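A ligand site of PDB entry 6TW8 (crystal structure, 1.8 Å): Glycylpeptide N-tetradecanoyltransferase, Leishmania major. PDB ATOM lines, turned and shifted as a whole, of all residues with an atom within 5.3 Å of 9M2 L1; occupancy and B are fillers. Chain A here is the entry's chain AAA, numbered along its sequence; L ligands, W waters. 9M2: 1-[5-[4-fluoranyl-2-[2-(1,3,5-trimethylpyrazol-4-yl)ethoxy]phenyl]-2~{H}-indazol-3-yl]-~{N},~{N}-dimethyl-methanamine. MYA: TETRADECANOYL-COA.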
ATOM      1  N   TYR A  77       3.373  18.667  35.800  1.00  0.00           N
ATOM      2  CA  TYR A  77       3.815  19.036  34.424  1.00  0.00           C
ATOM      3  C   TYR A  77       3.233  20.417  34.019  1.00  0.00           C
ATOM      4  O   TYR A  77       2.749  21.148  34.832  1.00  0.00           O
ATOM      5  CB  TYR A  77       3.679  17.840  33.475  1.00  0.00           C
ATOM      6  CG  TYR A  77       4.556  17.861  32.234  1.00  0.00           C
ATOM      7  CD1 TYR A  77       5.886  18.241  32.296  1.00  0.00           C
ATOM      8  CD2 TYR A  77       3.990  17.674  30.989  1.00  0.00           C
ATOM      9  CE1 TYR A  77       6.653  18.336  31.139  1.00  0.00           C
ATOM     10  CE2 TYR A  77       4.743  17.753  29.836  1.00  0.00           C
ATOM     11  CZ  TYR A  77       6.077  18.083  29.907  1.00  0.00           C
ATOM     12  OH  TYR A  77       6.793  18.164  28.763  1.00  0.00           O
ATOM     13  N   VAL A  78       3.349  20.738  32.750  1.00  0.00           N
ATOM     14  CA  VAL A  78       2.966  22.020  32.105  1.00  0.00           C
ATOM     15  C   VAL A  78       1.518  22.405  32.398  1.00  0.00           C
ATOM     16  O   VAL A  78       0.615  21.608  32.207  1.00  0.00           O
ATOM     17  CB  VAL A  78       3.226  21.975  30.595  1.00  0.00           C
ATOM     18  CG1 VAL A  78       2.867  23.285  29.927  1.00  0.00           C
ATOM     19  CG2 VAL A  78       4.666  21.598  30.282  1.00  0.00           C
ATOM     20  N   GLU A  79       1.403  23.644  32.868  1.00  0.00           N
ATOM     21  CA  GLU A  79       0.118  24.313  32.976  1.00  0.00           C
ATOM     22  C   GLU A  79       0.024  25.409  31.902  1.00  0.00           C
ATOM     23  O   GLU A  79       1.044  25.941  31.465  1.00  0.00           O
ATOM     24  CB  GLU A  79      -0.019  24.910  34.379  1.00  0.00           C
ATOM     25  CG  GLU A  79       0.032  23.846  35.442  1.00  0.00           C
ATOM     26  CD  GLU A  79      -0.085  24.324  36.886  1.00  0.00           C
ATOM     27  OE1 GLU A  79       0.016  23.444  37.788  1.00  0.00           O
ATOM     28  OE2 GLU A  79      -0.263  25.558  37.116  1.00  0.00           O
ATOM     29  N   ASP A  80      -1.201  25.776  31.507  1.00  0.00           N
ATOM     30  CA  ASP A  80      -1.364  26.837  30.523  1.00  0.00           C
ATOM     31  C   ASP A  80      -0.965  28.184  31.138  1.00  0.00           C
ATOM     32  O   ASP A  80      -0.822  28.308  32.354  1.00  0.00           O
ATOM     33  CB  ASP A  80      -2.800  26.923  30.008  1.00  0.00           C
ATOM     34  CG  ASP A  80      -3.715  27.406  31.124  1.00  0.00           C
ATOM     35  OD1 ASP A  80      -3.713  26.764  32.202  1.00  0.00           O
ATOM     36  OD2 ASP A  80      -4.421  28.430  30.905  1.00  0.00           O
ATOM     37  N   ASP A  81      -0.856  29.215  30.292  1.00  0.00           N
ATOM     38  CA  ASP A  81      -0.409  30.531  30.707  1.00  0.00           C
ATOM     39  C   ASP A  81      -1.289  31.124  31.813  1.00  0.00           C
ATOM     40  O   ASP A  81      -0.831  32.004  32.539  1.00  0.00           O
ATOM     41  CB  ASP A  81      -0.114  31.440  29.499  1.00  0.00           C
ATOM     42  CG  ASP A  81       1.145  31.031  28.756  1.00  0.00           C
ATOM     43  OD1 ASP A  81       1.925  30.237  29.337  1.00  0.00           O
ATOM     44  OD2 ASP A  81       1.355  31.489  27.583  1.00  0.00           O
ATOM     45  N   PHE A  85      -5.298  24.850  33.604  1.00  0.00           N
ATOM     46  CA  PHE A  85      -5.248  23.503  33.045  1.00  0.00           C
ATOM     47  C   PHE A  85      -3.837  22.933  33.188  1.00  0.00           C
ATOM     48  O   PHE A  85      -2.875  23.703  33.187  1.00  0.00           O
ATOM     49  CB  PHE A  85      -5.667  23.485  31.564  1.00  0.00           C
ATOM     50  CG  PHE A  85      -6.973  24.199  31.321  1.00  0.00           C
ATOM     51  CD1 PHE A  85      -8.163  23.716  31.824  1.00  0.00           C
ATOM     52  CD2 PHE A  85      -7.020  25.376  30.579  1.00  0.00           C
ATOM     53  CE1 PHE A  85      -9.346  24.407  31.641  1.00  0.00           C
ATOM     54  CE2 PHE A  85      -8.208  26.062  30.380  1.00  0.00           C
ATOM     55  CZ  PHE A  85      -9.375  25.581  30.926  1.00  0.00           C
ATOM     56  N   ARG A  86      -3.713  21.595  33.270  1.00  0.00           N
ATOM     57  CA  ARG A  86      -2.412  20.960  33.374  1.00  0.00           C
ATOM     58  C   ARG A  86      -2.398  19.696  32.524  1.00  0.00           C
ATOM     59  O   ARG A  86      -3.341  18.923  32.552  1.00  0.00           O
ATOM     60  CB  ARG A  86      -2.096  20.582  34.832  1.00  0.00           C
ATOM     61  CG  ARG A  86      -0.651  20.128  34.988  1.00  0.00           C
ATOM     62  CD  ARG A  86      -0.002  20.178  36.376  1.00  0.00           C
ATOM     63  NE  ARG A  86      -0.841  19.409  37.248  1.00  0.00           N
ATOM     64  CZ  ARG A  86      -1.502  19.861  38.299  1.00  0.00           C
ATOM     65  NH1 ARG A  86      -1.412  21.137  38.656  1.00  0.00           N
ATOM     66  NH2 ARG A  86      -2.257  19.033  38.975  1.00  0.00           N
ATOM     67  N   PHE A  87      -1.317  19.458  31.725  1.00  0.00           N
ATOM     68  CA  PHE A  87      -1.392  18.279  30.872  1.00  0.00           C
ATOM     69  C   PHE A  87      -1.472  17.003  31.704  1.00  0.00           C
ATOM     70  O   PHE A  87      -0.886  16.939  32.789  1.00  0.00           O
ATOM     71  CB  PHE A  87      -0.160  18.159  29.948  1.00  0.00           C
ATOM     72  CG  PHE A  87      -0.148  19.152  28.828  1.00  0.00           C
ATOM     73  CD1 PHE A  87      -1.292  19.389  28.066  1.00  0.00           C
ATOM     74  CD2 PHE A  87       1.042  19.796  28.497  1.00  0.00           C
ATOM     75  CE1 PHE A  87      -1.250  20.267  26.995  1.00  0.00           C
ATOM     76  CE2 PHE A  87       1.050  20.718  27.446  1.00  0.00           C
ATOM     77  CZ  PHE A  87      -0.070  20.932  26.692  1.00  0.00           C
ATOM     78  N   TYR A  89      -0.878  13.502  30.375  1.00  0.00           N
ATOM     79  CA  TYR A  89      -0.596  12.476  29.388  1.00  0.00           C
ATOM     80  C   TYR A  89      -0.849  11.103  30.008  1.00  0.00           C
ATOM     81  O   TYR A  89      -0.512  10.850  31.175  1.00  0.00           O
ATOM     82  CB  TYR A  89       0.872  12.519  28.947  1.00  0.00           C
ATOM     83  CG  TYR A  89       1.308  13.762  28.204  1.00  0.00           C
ATOM     84  CD1 TYR A  89       1.541  14.972  28.859  1.00  0.00           C
ATOM     85  CD2 TYR A  89       1.526  13.716  26.828  1.00  0.00           C
ATOM     86  CE1 TYR A  89       2.014  16.096  28.171  1.00  0.00           C
ATOM     87  CE2 TYR A  89       1.966  14.826  26.116  1.00  0.00           C
ATOM     88  CZ  TYR A  89       2.210  16.014  26.794  1.00  0.00           C
ATOM     89  OH  TYR A  89       2.635  17.089  26.074  1.00  0.00           O
ATOM     90  N   ASN A 164      12.182  16.207  25.823  1.00  0.00           N
ATOM     91  CA  ASN A 164      10.795  16.476  26.164  1.00  0.00           C
ATOM     92  C   ASN A 164      10.590  15.968  27.587  1.00  0.00           C
ATOM     93  O   ASN A 164      11.441  15.253  28.126  1.00  0.00           O
ATOM     94  CB  ASN A 164       9.901  15.727  25.173  1.00  0.00           C
ATOM     95  CG  ASN A 164       8.525  16.327  24.977  1.00  0.00           C
ATOM     96  OD1 ASN A 164       8.080  17.148  25.759  1.00  0.00           O
ATOM     97  ND2 ASN A 164       7.878  15.936  23.896  1.00  0.00           N
ATOM     98  N   THR A 200      11.175  22.006  22.325  1.00  0.00           N
ATOM     99  CA  THR A 200      10.195  23.069  22.269  1.00  0.00           C
ATOM    100  C   THR A 200       9.814  23.429  23.712  1.00  0.00           C
ATOM    101  O   THR A 200       9.988  22.617  24.614  1.00  0.00           O
ATOM    102  CB  THR A 200       8.935  22.646  21.491  1.00  0.00           C
ATOM    103  OG1 THR A 200       8.506  21.349  21.877  1.00  0.00           O
ATOM    104  CG2 THR A 200       9.151  22.582  20.001  1.00  0.00           C
ATOM    105  N   ALA A 201       9.378  24.680  23.931  1.00  0.00           N
ATOM    106  CA  ALA A 201       8.813  25.069  25.216  1.00  0.00           C
ATOM    107  C   ALA A 201       7.870  26.237  24.974  1.00  0.00           C
ATOM    108  O   ALA A 201       7.993  26.928  23.975  1.00  0.00           O
ATOM    109  CB  ALA A 201       9.878  25.495  26.211  1.00  0.00           C
ATOM    110  N   GLY A 202       6.904  26.408  25.896  1.00  0.00           N
ATOM    111  CA  GLY A 202       6.003  27.544  25.855  1.00  0.00           C
ATOM    112  C   GLY A 202       6.612  28.792  26.492  1.00  0.00           C
ATOM    113  O   GLY A 202       5.972  29.841  26.524  1.00  0.00           O
ATOM    114  N   TYR A 214      -0.286  29.079  19.220  1.00  0.00           N
ATOM    115  CA  TYR A 214      -1.182  27.951  19.097  1.00  0.00           C
ATOM    116  C   TYR A 214      -2.606  28.444  18.825  1.00  0.00           C
ATOM    117  O   TYR A 214      -2.930  29.612  19.090  1.00  0.00           O
ATOM    118  CB  TYR A 214      -1.051  27.010  20.296  1.00  0.00           C
ATOM    119  CG  TYR A 214      -1.765  27.488  21.531  1.00  0.00           C
ATOM    120  CD1 TYR A 214      -3.132  27.337  21.669  1.00  0.00           C
ATOM    121  CD2 TYR A 214      -1.073  28.080  22.574  1.00  0.00           C
ATOM    122  CE1 TYR A 214      -3.805  27.764  22.801  1.00  0.00           C
ATOM    123  CE2 TYR A 214      -1.729  28.508  23.720  1.00  0.00           C
ATOM    124  CZ  TYR A 214      -3.101  28.355  23.828  1.00  0.00           C
ATOM    125  OH  TYR A 214      -3.772  28.773  24.950  1.00  0.00           O
ATOM    126  N   PHE A 215      -3.435  27.529  18.285  1.00  0.00           N
ATOM    127  CA  PHE A 215      -4.784  27.843  17.824  1.00  0.00           C
ATOM    128  C   PHE A 215      -5.708  26.756  18.348  1.00  0.00           C
ATOM    129  O   PHE A 215      -5.293  25.603  18.521  1.00  0.00           O
ATOM    130  CB  PHE A 215      -4.846  27.808  16.305  1.00  0.00           C
ATOM    131  CG  PHE A 215      -4.241  29.032  15.658  1.00  0.00           C
ATOM    132  CD1 PHE A 215      -2.864  29.191  15.616  1.00  0.00           C
ATOM    133  CD2 PHE A 215      -5.057  30.020  15.129  1.00  0.00           C
ATOM    134  CE1 PHE A 215      -2.313  30.335  15.076  1.00  0.00           C
ATOM    135  CE2 PHE A 215      -4.499  31.158  14.556  1.00  0.00           C
ATOM    136  CZ  PHE A 215      -3.130  31.305  14.534  1.00  0.00           C
ATOM    137  N   PHE A 229     -12.428  27.388  29.558  1.00  0.00           N
ATOM    138  CA  PHE A 229     -11.465  27.393  28.462  1.00  0.00           C
ATOM    139  C   PHE A 229     -11.855  28.469  27.465  1.00  0.00           C
ATOM    140  O   PHE A 229     -10.969  29.155  26.957  1.00  0.00           O
ATOM    141  CB  PHE A 229     -11.368  26.021  27.777  1.00  0.00           C
ATOM    142  CG  PHE A 229     -10.466  25.958  26.565  1.00  0.00           C
ATOM    143  CD1 PHE A 229     -10.939  26.240  25.289  1.00  0.00           C
ATOM    144  CD2 PHE A 229      -9.142  25.543  26.687  1.00  0.00           C
ATOM    145  CE1 PHE A 229     -10.111  26.129  24.178  1.00  0.00           C
ATOM    146  CE2 PHE A 229      -8.314  25.432  25.576  1.00  0.00           C
ATOM    147  CZ  PHE A 229      -8.801  25.726  24.326  1.00  0.00           C
ATOM    148  N   SER A 327      -6.250  17.561  29.430  1.00  0.00           N
ATOM    149  CA  SER A 327      -5.773  18.489  30.446  1.00  0.00           C
ATOM    150  C   SER A 327      -6.668  18.388  31.681  1.00  0.00           C
ATOM    151  O   SER A 327      -7.878  18.442  31.549  1.00  0.00           O
ATOM    152  CB  SER A 327      -5.680  19.919  29.937  1.00  0.00           C
ATOM    153  OG  SER A 327      -4.571  20.071  29.039  1.00  0.00           O
ATOM    154  N   LEU A 338     -10.319  18.536  30.075  1.00  0.00           N
ATOM    155  CA  LEU A 338     -10.411  19.078  28.734  1.00  0.00           C
ATOM    156  C   LEU A 338      -9.865  18.008  27.817  1.00  0.00           C
ATOM    157  O   LEU A 338      -8.701  17.651  27.948  1.00  0.00           O
ATOM    158  CB  LEU A 338      -9.554  20.334  28.622  1.00  0.00           C
ATOM    159  CG  LEU A 338      -9.459  20.859  27.187  1.00  0.00           C
ATOM    160  CD1 LEU A 338     -10.751  21.563  26.816  1.00  0.00           C
ATOM    161  CD2 LEU A 338      -8.255  21.765  27.003  1.00  0.00           C
ATOM    162  N   TYR A 342      -4.820  16.967  19.217  1.00  0.00           N
ATOM    163  CA  TYR A 342      -3.777  17.830  18.658  1.00  0.00           C
ATOM    164  C   TYR A 342      -3.546  17.423  17.219  1.00  0.00           C
ATOM    165  O   TYR A 342      -3.384  16.241  16.944  1.00  0.00           O
ATOM    166  CB  TYR A 342      -2.490  17.799  19.509  1.00  0.00           C
ATOM    167  CG  TYR A 342      -2.689  18.439  20.846  1.00  0.00           C
ATOM    168  CD1 TYR A 342      -3.358  17.785  21.862  1.00  0.00           C
ATOM    169  CD2 TYR A 342      -2.289  19.756  21.058  1.00  0.00           C
ATOM    170  CE1 TYR A 342      -3.579  18.417  23.081  1.00  0.00           C
ATOM    171  CE2 TYR A 342      -2.507  20.400  22.265  1.00  0.00           C
ATOM    172  CZ  TYR A 342      -3.221  19.738  23.260  1.00  0.00           C
ATOM    173  OH  TYR A 342      -3.458  20.385  24.440  1.00  0.00           O
ATOM    174  N   ASN A 373      -6.502  21.412  18.896  1.00  0.00           N
ATOM    175  CA  ASN A 373      -5.408  22.363  19.116  1.00  0.00           C
ATOM    176  C   ASN A 373      -4.316  22.128  18.084  1.00  0.00           C
ATOM    177  O   ASN A 373      -4.144  21.034  17.553  1.00  0.00           O
ATOM    178  CB  ASN A 373      -4.805  22.240  20.514  1.00  0.00           C
ATOM    179  CG  ASN A 373      -5.756  22.753  21.574  1.00  0.00           C
ATOM    180  OD1 ASN A 373      -6.680  23.506  21.253  1.00  0.00           O
ATOM    181  ND2 ASN A 373      -5.533  22.345  22.809  1.00  0.00           N
ATOM    182  N   MET A 374      -3.607  23.219  17.762  1.00  0.00           N
ATOM    183  CA  MET A 374      -2.434  23.075  16.909  1.00  0.00           C
ATOM    184  C   MET A 374      -1.541  24.296  17.070  1.00  0.00           C
ATOM    185  O   MET A 374      -1.981  25.289  17.633  1.00  0.00           O
ATOM    186  CB  MET A 374      -2.813  22.950  15.421  1.00  0.00           C
ATOM    187  CG  MET A 374      -3.515  24.177  14.852  1.00  0.00           C
ATOM    188  SD  MET A 374      -4.091  23.876  13.154  1.00  0.00           S
ATOM    189  CE  MET A 374      -4.649  25.556  12.810  1.00  0.00           C
ATOM    190  N   VAL A 375      -0.311  24.182  16.602  1.00  0.00           N
ATOM    191  CA  VAL A 375       0.627  25.335  16.539  1.00  0.00           C
ATOM    192  C   VAL A 375       0.610  25.751  15.068  1.00  0.00           C
ATOM    193  O   VAL A 375       0.462  24.886  14.212  1.00  0.00           O
ATOM    194  CB  VAL A 375       2.036  24.937  17.005  1.00  0.00           C
ATOM    195  CG1 VAL A 375       3.041  26.079  16.957  1.00  0.00           C
ATOM    196  CG2 VAL A 375       2.004  24.310  18.373  1.00  0.00           C
ATOM    197  N   LEU A 396       4.474  28.413  21.175  1.00  0.00           N
ATOM    198  CA  LEU A 396       5.423  27.328  21.285  1.00  0.00           C
ATOM    199  C   LEU A 396       6.697  27.753  20.536  1.00  0.00           C
ATOM    200  O   LEU A 396       6.636  28.095  19.369  1.00  0.00           O
ATOM    201  CB  LEU A 396       4.824  26.006  20.804  1.00  0.00           C
ATOM    202  CG  LEU A 396       5.686  24.776  21.130  1.00  0.00           C
ATOM    203  CD1 LEU A 396       5.567  24.389  22.594  1.00  0.00           C
ATOM    204  CD2 LEU A 396       5.375  23.573  20.210  1.00  0.00           C
ATOM    205  N   MET A 417       6.104  18.439  17.849  1.00  0.00           N
ATOM    206  CA  MET A 417       6.563  17.896  19.118  1.00  0.00           C
ATOM    207  C   MET A 417       5.378  17.685  20.078  1.00  0.00           C
ATOM    208  O   MET A 417       4.452  18.526  20.204  1.00  0.00           O
ATOM    209  CB  MET A 417       7.703  18.739  19.718  1.00  0.00           C
ATOM    210  CG  MET A 417       9.026  18.334  19.075  1.00  0.00           C
ATOM    211  SD  MET A 417      10.495  18.827  19.970  1.00  0.00           S
ATOM    212  CE  MET A 417      10.757  20.381  19.133  1.00  0.00           C
ATOM    213  N   LEU A 418       5.449  16.509  20.724  1.00  0.00           N
ATOM    214  CA  LEU A 418       4.384  15.992  21.570  1.00  0.00           C
ATOM    215  C   LEU A 418       4.443  16.666  22.938  1.00  0.00           C
ATOM    216  O   LEU A 418       5.472  17.149  23.466  1.00  0.00           O
ATOM    217  CB  LEU A 418       4.542  14.471  21.699  1.00  0.00           C
ATOM    218  CG  LEU A 418       4.517  13.636  20.427  1.00  0.00           C
ATOM    219  CD1 LEU A 418       4.752  12.165  20.776  1.00  0.00           C
ATOM    220  CD2 LEU A 418       3.207  13.772  19.648  1.00  0.00           C
ATOM    221  OXT LEU A 418       3.407  16.726  23.601  1.00  0.00           O
HETATM  222  C12 9M2 L   1       0.403  22.742  20.968  1.00  0.00           C
HETATM  223  C8  9M2 L   1       2.761  22.412  24.579  1.00  0.00           C
HETATM  224  C9  9M2 L   1       3.752  22.551  25.511  1.00  0.00           C
HETATM  225  C10 9M2 L   1       0.874  23.415  23.241  1.00  0.00           C
HETATM  226  C11 9M2 L   1       1.279  22.891  22.026  1.00  0.00           C
HETATM  227  C7  9M2 L   1       1.935  23.501  24.310  1.00  0.00           C
HETATM  228  C6  9M2 L   1       2.132  24.716  25.012  1.00  0.00           C
HETATM  229  N1  9M2 L   1       5.464  22.271  26.911  1.00  0.00           N
HETATM  230  C5  9M2 L   1       3.148  24.905  25.970  1.00  0.00           C
HETATM  231  C4  9M2 L   1       3.965  23.798  26.235  1.00  0.00           C
HETATM  232  F   9M2 L   1      -1.623  23.154  19.984  1.00  0.00           F
HETATM  233  C13 9M2 L   1      -0.863  23.237  21.061  1.00  0.00           C
HETATM  234  C14 9M2 L   1      -1.353  23.860  22.211  1.00  0.00           C
HETATM  235  C15 9M2 L   1      -0.478  23.960  23.286  1.00  0.00           C
HETATM  236  N2  9M2 L   1       5.018  23.569  27.040  1.00  0.00           N
HETATM  237  C3  9M2 L   1       4.739  21.589  26.030  1.00  0.00           C
HETATM  238  C2  9M2 L   1       4.940  20.113  25.642  1.00  0.00           C
HETATM  239  N   9M2 L   1       5.841  19.780  24.485  1.00  0.00           N
HETATM  240  C1  9M2 L   1       5.301  20.316  23.255  1.00  0.00           C
HETATM  241  C   9M2 L   1       7.214  20.201  24.767  1.00  0.00           C
HETATM  242  O   9M2 L   1      -0.895  24.513  24.400  1.00  0.00           O
HETATM  243  C16 9M2 L   1      -2.293  24.777  24.492  1.00  0.00           C
HETATM  244  C17 9M2 L   1      -2.512  25.372  25.869  1.00  0.00           C
HETATM  245  C18 9M2 L   1      -2.643  24.335  26.977  1.00  0.00           C
HETATM  246  C22 9M2 L   1      -3.809  23.440  27.279  1.00  0.00           C
HETATM  247  C23 9M2 L   1      -5.101  23.329  26.517  1.00  0.00           C
HETATM  248  N4  9M2 L   1      -3.471  22.718  28.348  1.00  0.00           N
HETATM  249  N3  9M2 L   1      -2.170  23.092  28.731  1.00  0.00           N
HETATM  250  C21 9M2 L   1      -1.596  22.397  29.904  1.00  0.00           C
HETATM  251  C19 9M2 L   1      -1.640  24.030  28.007  1.00  0.00           C
HETATM  252  C20 9M2 L   1      -0.243  24.534  28.273  1.00  0.00           C
HETATM  253  S1  MYA L   2       9.385  21.944  27.807  1.00  0.00           S
HETATM  254  C2  MYA L   2       8.362  21.397  29.184  1.00  0.00           C
HETATM  255  C3  MYA L   2       8.918  22.069  30.429  1.00  0.00           C
HETATM  256  N4  MYA L   2       8.239  21.514  31.617  1.00  0.00           N
HETATM  257  C5  MYA L   2       7.396  22.236  32.381  1.00  0.00           C
HETATM  258  O5  MYA L   2       7.141  23.393  32.128  1.00  0.00           O
HETATM  259  C6  MYA L   2       6.742  21.539  33.554  1.00  0.00           C
HETATM  260  C7  MYA L   2       6.417  22.516  34.691  1.00  0.00           C
HETATM  261  N8  MYA L   2       7.655  23.152  35.174  1.00  0.00           N
HETATM  262  C9  MYA L   2       8.640  22.555  35.765  1.00  0.00           C
HETATM  263  O9  MYA L   2       8.642  21.315  35.996  1.00  0.00           O
HETATM  264  C10 MYA L   2       9.822  23.396  36.194  1.00  0.00           C
HETATM  265  O10 MYA L   2       9.440  24.809  36.284  1.00  0.00           O
HETATM  266  C11 MYA L   2      11.039  23.291  35.232  1.00  0.00           C
HETATM  267  C12 MYA L   2      12.135  24.287  35.639  1.00  0.00           C
HETATM  268  C13 MYA L   2      10.530  23.632  33.819  1.00  0.00           C
HETATM  269  C14 MYA L   2      11.595  21.871  35.277  1.00  0.00           C
HETATM  270  N1A MYA L   2      13.393  24.353  29.376  1.00  0.00           N
HETATM  271  O1A MYA L   2      15.496  24.079  38.591  1.00  0.00           O
HETATM  272  P1A MYA L   2      15.288  25.558  38.301  1.00  0.00           P
HETATM  273  C1X MYA L   2      15.580  27.189  33.067  1.00  0.00           C
HETATM  274  C2A MYA L   2      14.681  24.680  29.551  1.00  0.00           C
HETATM  275  O2A MYA L   2      15.667  26.559  39.384  1.00  0.00           O
HETATM  276  P2A MYA L   2      12.479  25.110  38.089  1.00  0.00           P
HETATM  277  C2M MYA L   2      10.496  20.663  27.733  1.00  0.00           C
HETATM  278  O2M MYA L   2      10.256  19.611  28.340  1.00  0.00           O
HETATM  279  C2X MYA L   2      15.514  28.614  33.516  1.00  0.00           C
HETATM  280  O2X MYA L   2      15.629  29.509  32.423  1.00  0.00           O
HETATM  281  N3A MYA L   2      15.088  25.411  30.585  1.00  0.00           N
HETATM  282  O3A MYA L   2      13.825  25.962  37.818  1.00  0.00           O
HETATM  283  C3M MYA L   2      11.769  20.762  26.893  1.00  0.00           C
HETATM  284  C3X MYA L   2      16.682  28.697  34.490  1.00  0.00           C
HETATM  285  O3X MYA L   2      17.945  28.870  33.786  1.00  0.00           O
HETATM  286  P3X MYA L   2      18.689  30.266  33.672  1.00  0.00           P
HETATM  287  C4A MYA L   2      14.172  25.901  31.432  1.00  0.00           C
HETATM  288  O4A MYA L   2      11.375  26.068  37.758  1.00  0.00           O
HETATM  289  C4M MYA L   2      12.929  20.881  27.870  1.00  0.00           C
HETATM  290  C4X MYA L   2      16.679  27.315  35.101  1.00  0.00           C
HETATM  291  O4X MYA L   2      15.875  26.447  34.257  1.00  0.00           O
HETATM  292  C5A MYA L   2      12.809  25.621  31.245  1.00  0.00           C
HETATM  293  O5A MYA L   2      12.481  24.468  39.409  1.00  0.00           O
HETATM  294  C5M MYA L   2      14.199  21.242  27.162  1.00  0.00           C
HETATM  295  C5X MYA L   2      16.083  27.301  36.496  1.00  0.00           C
HETATM  296  O5X MYA L   2      16.151  25.973  37.030  1.00  0.00           O
HETATM  297  C6A MYA L   2      12.432  24.831  30.164  1.00  0.00           C
HETATM  298  N6A MYA L   2      11.123  24.547  29.891  1.00  0.00           N
HETATM  299  O6A MYA L   2      12.596  23.974  36.974  1.00  0.00           O
HETATM  300  C6M MYA L   2      15.357  21.316  28.193  1.00  0.00           C
HETATM  301  N7A MYA L   2      12.106  26.242  32.230  1.00  0.00           N
HETATM  302  O7A MYA L   2      17.603  31.139  33.047  1.00  0.00           O
HETATM  303  C7M MYA L   2      16.653  21.826  27.516  1.00  0.00           C
HETATM  304  C8A MYA L   2      13.044  26.874  33.014  1.00  0.00           C
HETATM  305  O8A MYA L   2      18.901  30.584  35.123  1.00  0.00           O
HETATM  306  C8M MYA L   2      17.456  20.630  26.940  1.00  0.00           C
HETATM  307  N9A MYA L   2      14.281  26.699  32.508  1.00  0.00           N
HETATM  308  O9A MYA L   2      19.896  30.098  32.760  1.00  0.00           O
HETATM  309  C9M MYA L   2      18.709  21.123  26.128  1.00  0.00           C
HETATM  310  CAM MYA L   2      19.375  19.987  25.312  1.00  0.00           C
HETATM  311  CBM MYA L   2      19.711  18.730  26.135  1.00  0.00           C
HETATM  312  CCM MYA L   2      20.312  17.541  25.338  1.00  0.00           C
HETATM  313  CDM MYA L   2      21.567  17.915  24.503  1.00  0.00           C
HETATM  314  CEM MYA L   2      22.148  16.598  23.908  1.00  0.00           C
HETATM  315  CFM MYA L   2      23.219  16.896  22.838  1.00  0.00           C
HETATM  316  O   HOH W   1       1.599  27.827  26.801  1.00  0.00           O
HETATM  317  O   HOH W   2       6.736  25.313  28.673  1.00  0.00           O
HETATM  318  O   HOH W   3       5.537  17.486  26.567  1.00  0.00           O
HETATM  319  O   HOH W   4      10.309  19.581  23.732  1.00  0.00           O
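The chain-end carboxylate of Leu 418 is in salt-bridge range of a nitrogen (N) of 9M2 L1 (2.8 Å).
N4 of 9M2 L1 lies within hydrogen-bond range of OG of Ser 327 (2.9 Å).
The backbone NH of Met 374 lies close to a fluorine (F) of 9M2 L1 (3.0 Å).
Val 78 touches 9M2 L1 (O to C21, 3.3 Å).
Glu 79 touches 9M2 L1.
Asp 80 touches 9M2 L1 (CA to C20, 3.4 Å).
Phe 85 touches 9M2 L1.
Arg 86 touches 9M2 L1.
Phe 87 touches 9M2 L1 (CE1 to N3, 3.4 Å).
OH of Tyr 89 touches C2 of 9M2 L1, at 3.8 Å.
OD1 of Asn 164 touches C of 9M2 L1, 3.3 Å away.
Thr 200 touches 9M2 L1.
Gly 202 touches 9M2 L1 (N to N2, 3.6 Å).
CZ of Tyr 214 touches C17 of 9M2 L1 (3.7 Å).
Phe 229 touches 9M2 L1 (CE2 to C23, 3.95 Å).
Leu 338 touches 9M2 L1.
Tyr 342 touches 9M2 L1 (CE2 to C13, 3.5 Å).
CB of Asn 373 touches F of 9M2 L1, 3.4 Å away.
Val 375 touches 9M2 L1 (CG2 to C12, 3.4 Å).
Leu 396 touches 9M2 L1 (CD1 to C9, 3.9 Å).
Met 417 touches 9M2 L1 (O to C1, 3.6 Å).
Hydrophobic or aromatic side chains within 4 Å of 9M2 L1: Val 78, Phe 85, Phe 87, Tyr 214, Phe 229, Leu 338, Tyr 342, Val 375 and Leu 396.
21 residues have an atom within 4 Å of 9M2 L1: Val 78, Glu 79, Asp 80, Phe 85, Arg 86, Phe 87, Tyr 89, Asn 164, Thr 200, Gly 202, Tyr 214, Phe 229, Ser 327, Leu 338, Tyr 342, Asn 373, Met 374, Val 375, Leu 396, Met 417 and Leu 418.
Water W3 lies within hydrogen-bond range of OH of Tyr 77, OD1 of Asn 164, OH of Tyr 89 and O of Leu 418.
Water W2 lies within hydrogen-bond range of N2 of 9M2 L1 and N of Gly 202.
The backbone carbonyl oxygen (O) of Ser 327 lies within hydrogen-bond range of the backbone NH (N) of Leu 338.
The backbone NH of Phe 215 sits at hydrogen-bond distance from the backbone carbonyl oxygen of Met 374, 2.7 Å away.
The backbone carbonyl oxygen of Val 78 is in hydrogen-bond range of the backbone NH of Phe 87 (2.9 Å).
OD1 of Asn 164 is in hydrogen-bond range of OH of Tyr 77 (3.4 Å).
The side-chain amide nitrogen of Asn 373 lies within hydrogen-bond range of the side-chain hydroxyl of Tyr 342.
The side-chain hydroxyl (OG1) of Thr 200 lies close to the side-chain sulfur (SD) of Met 417 (3.7 Å).
OD1 of Asp 80 is in hydrogen-bond range of N of Phe 85.
The side-chain carboxylate of Glu 79 lies within salt-bridge range of the guanidinium group of Arg 86 (2.8 Å).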
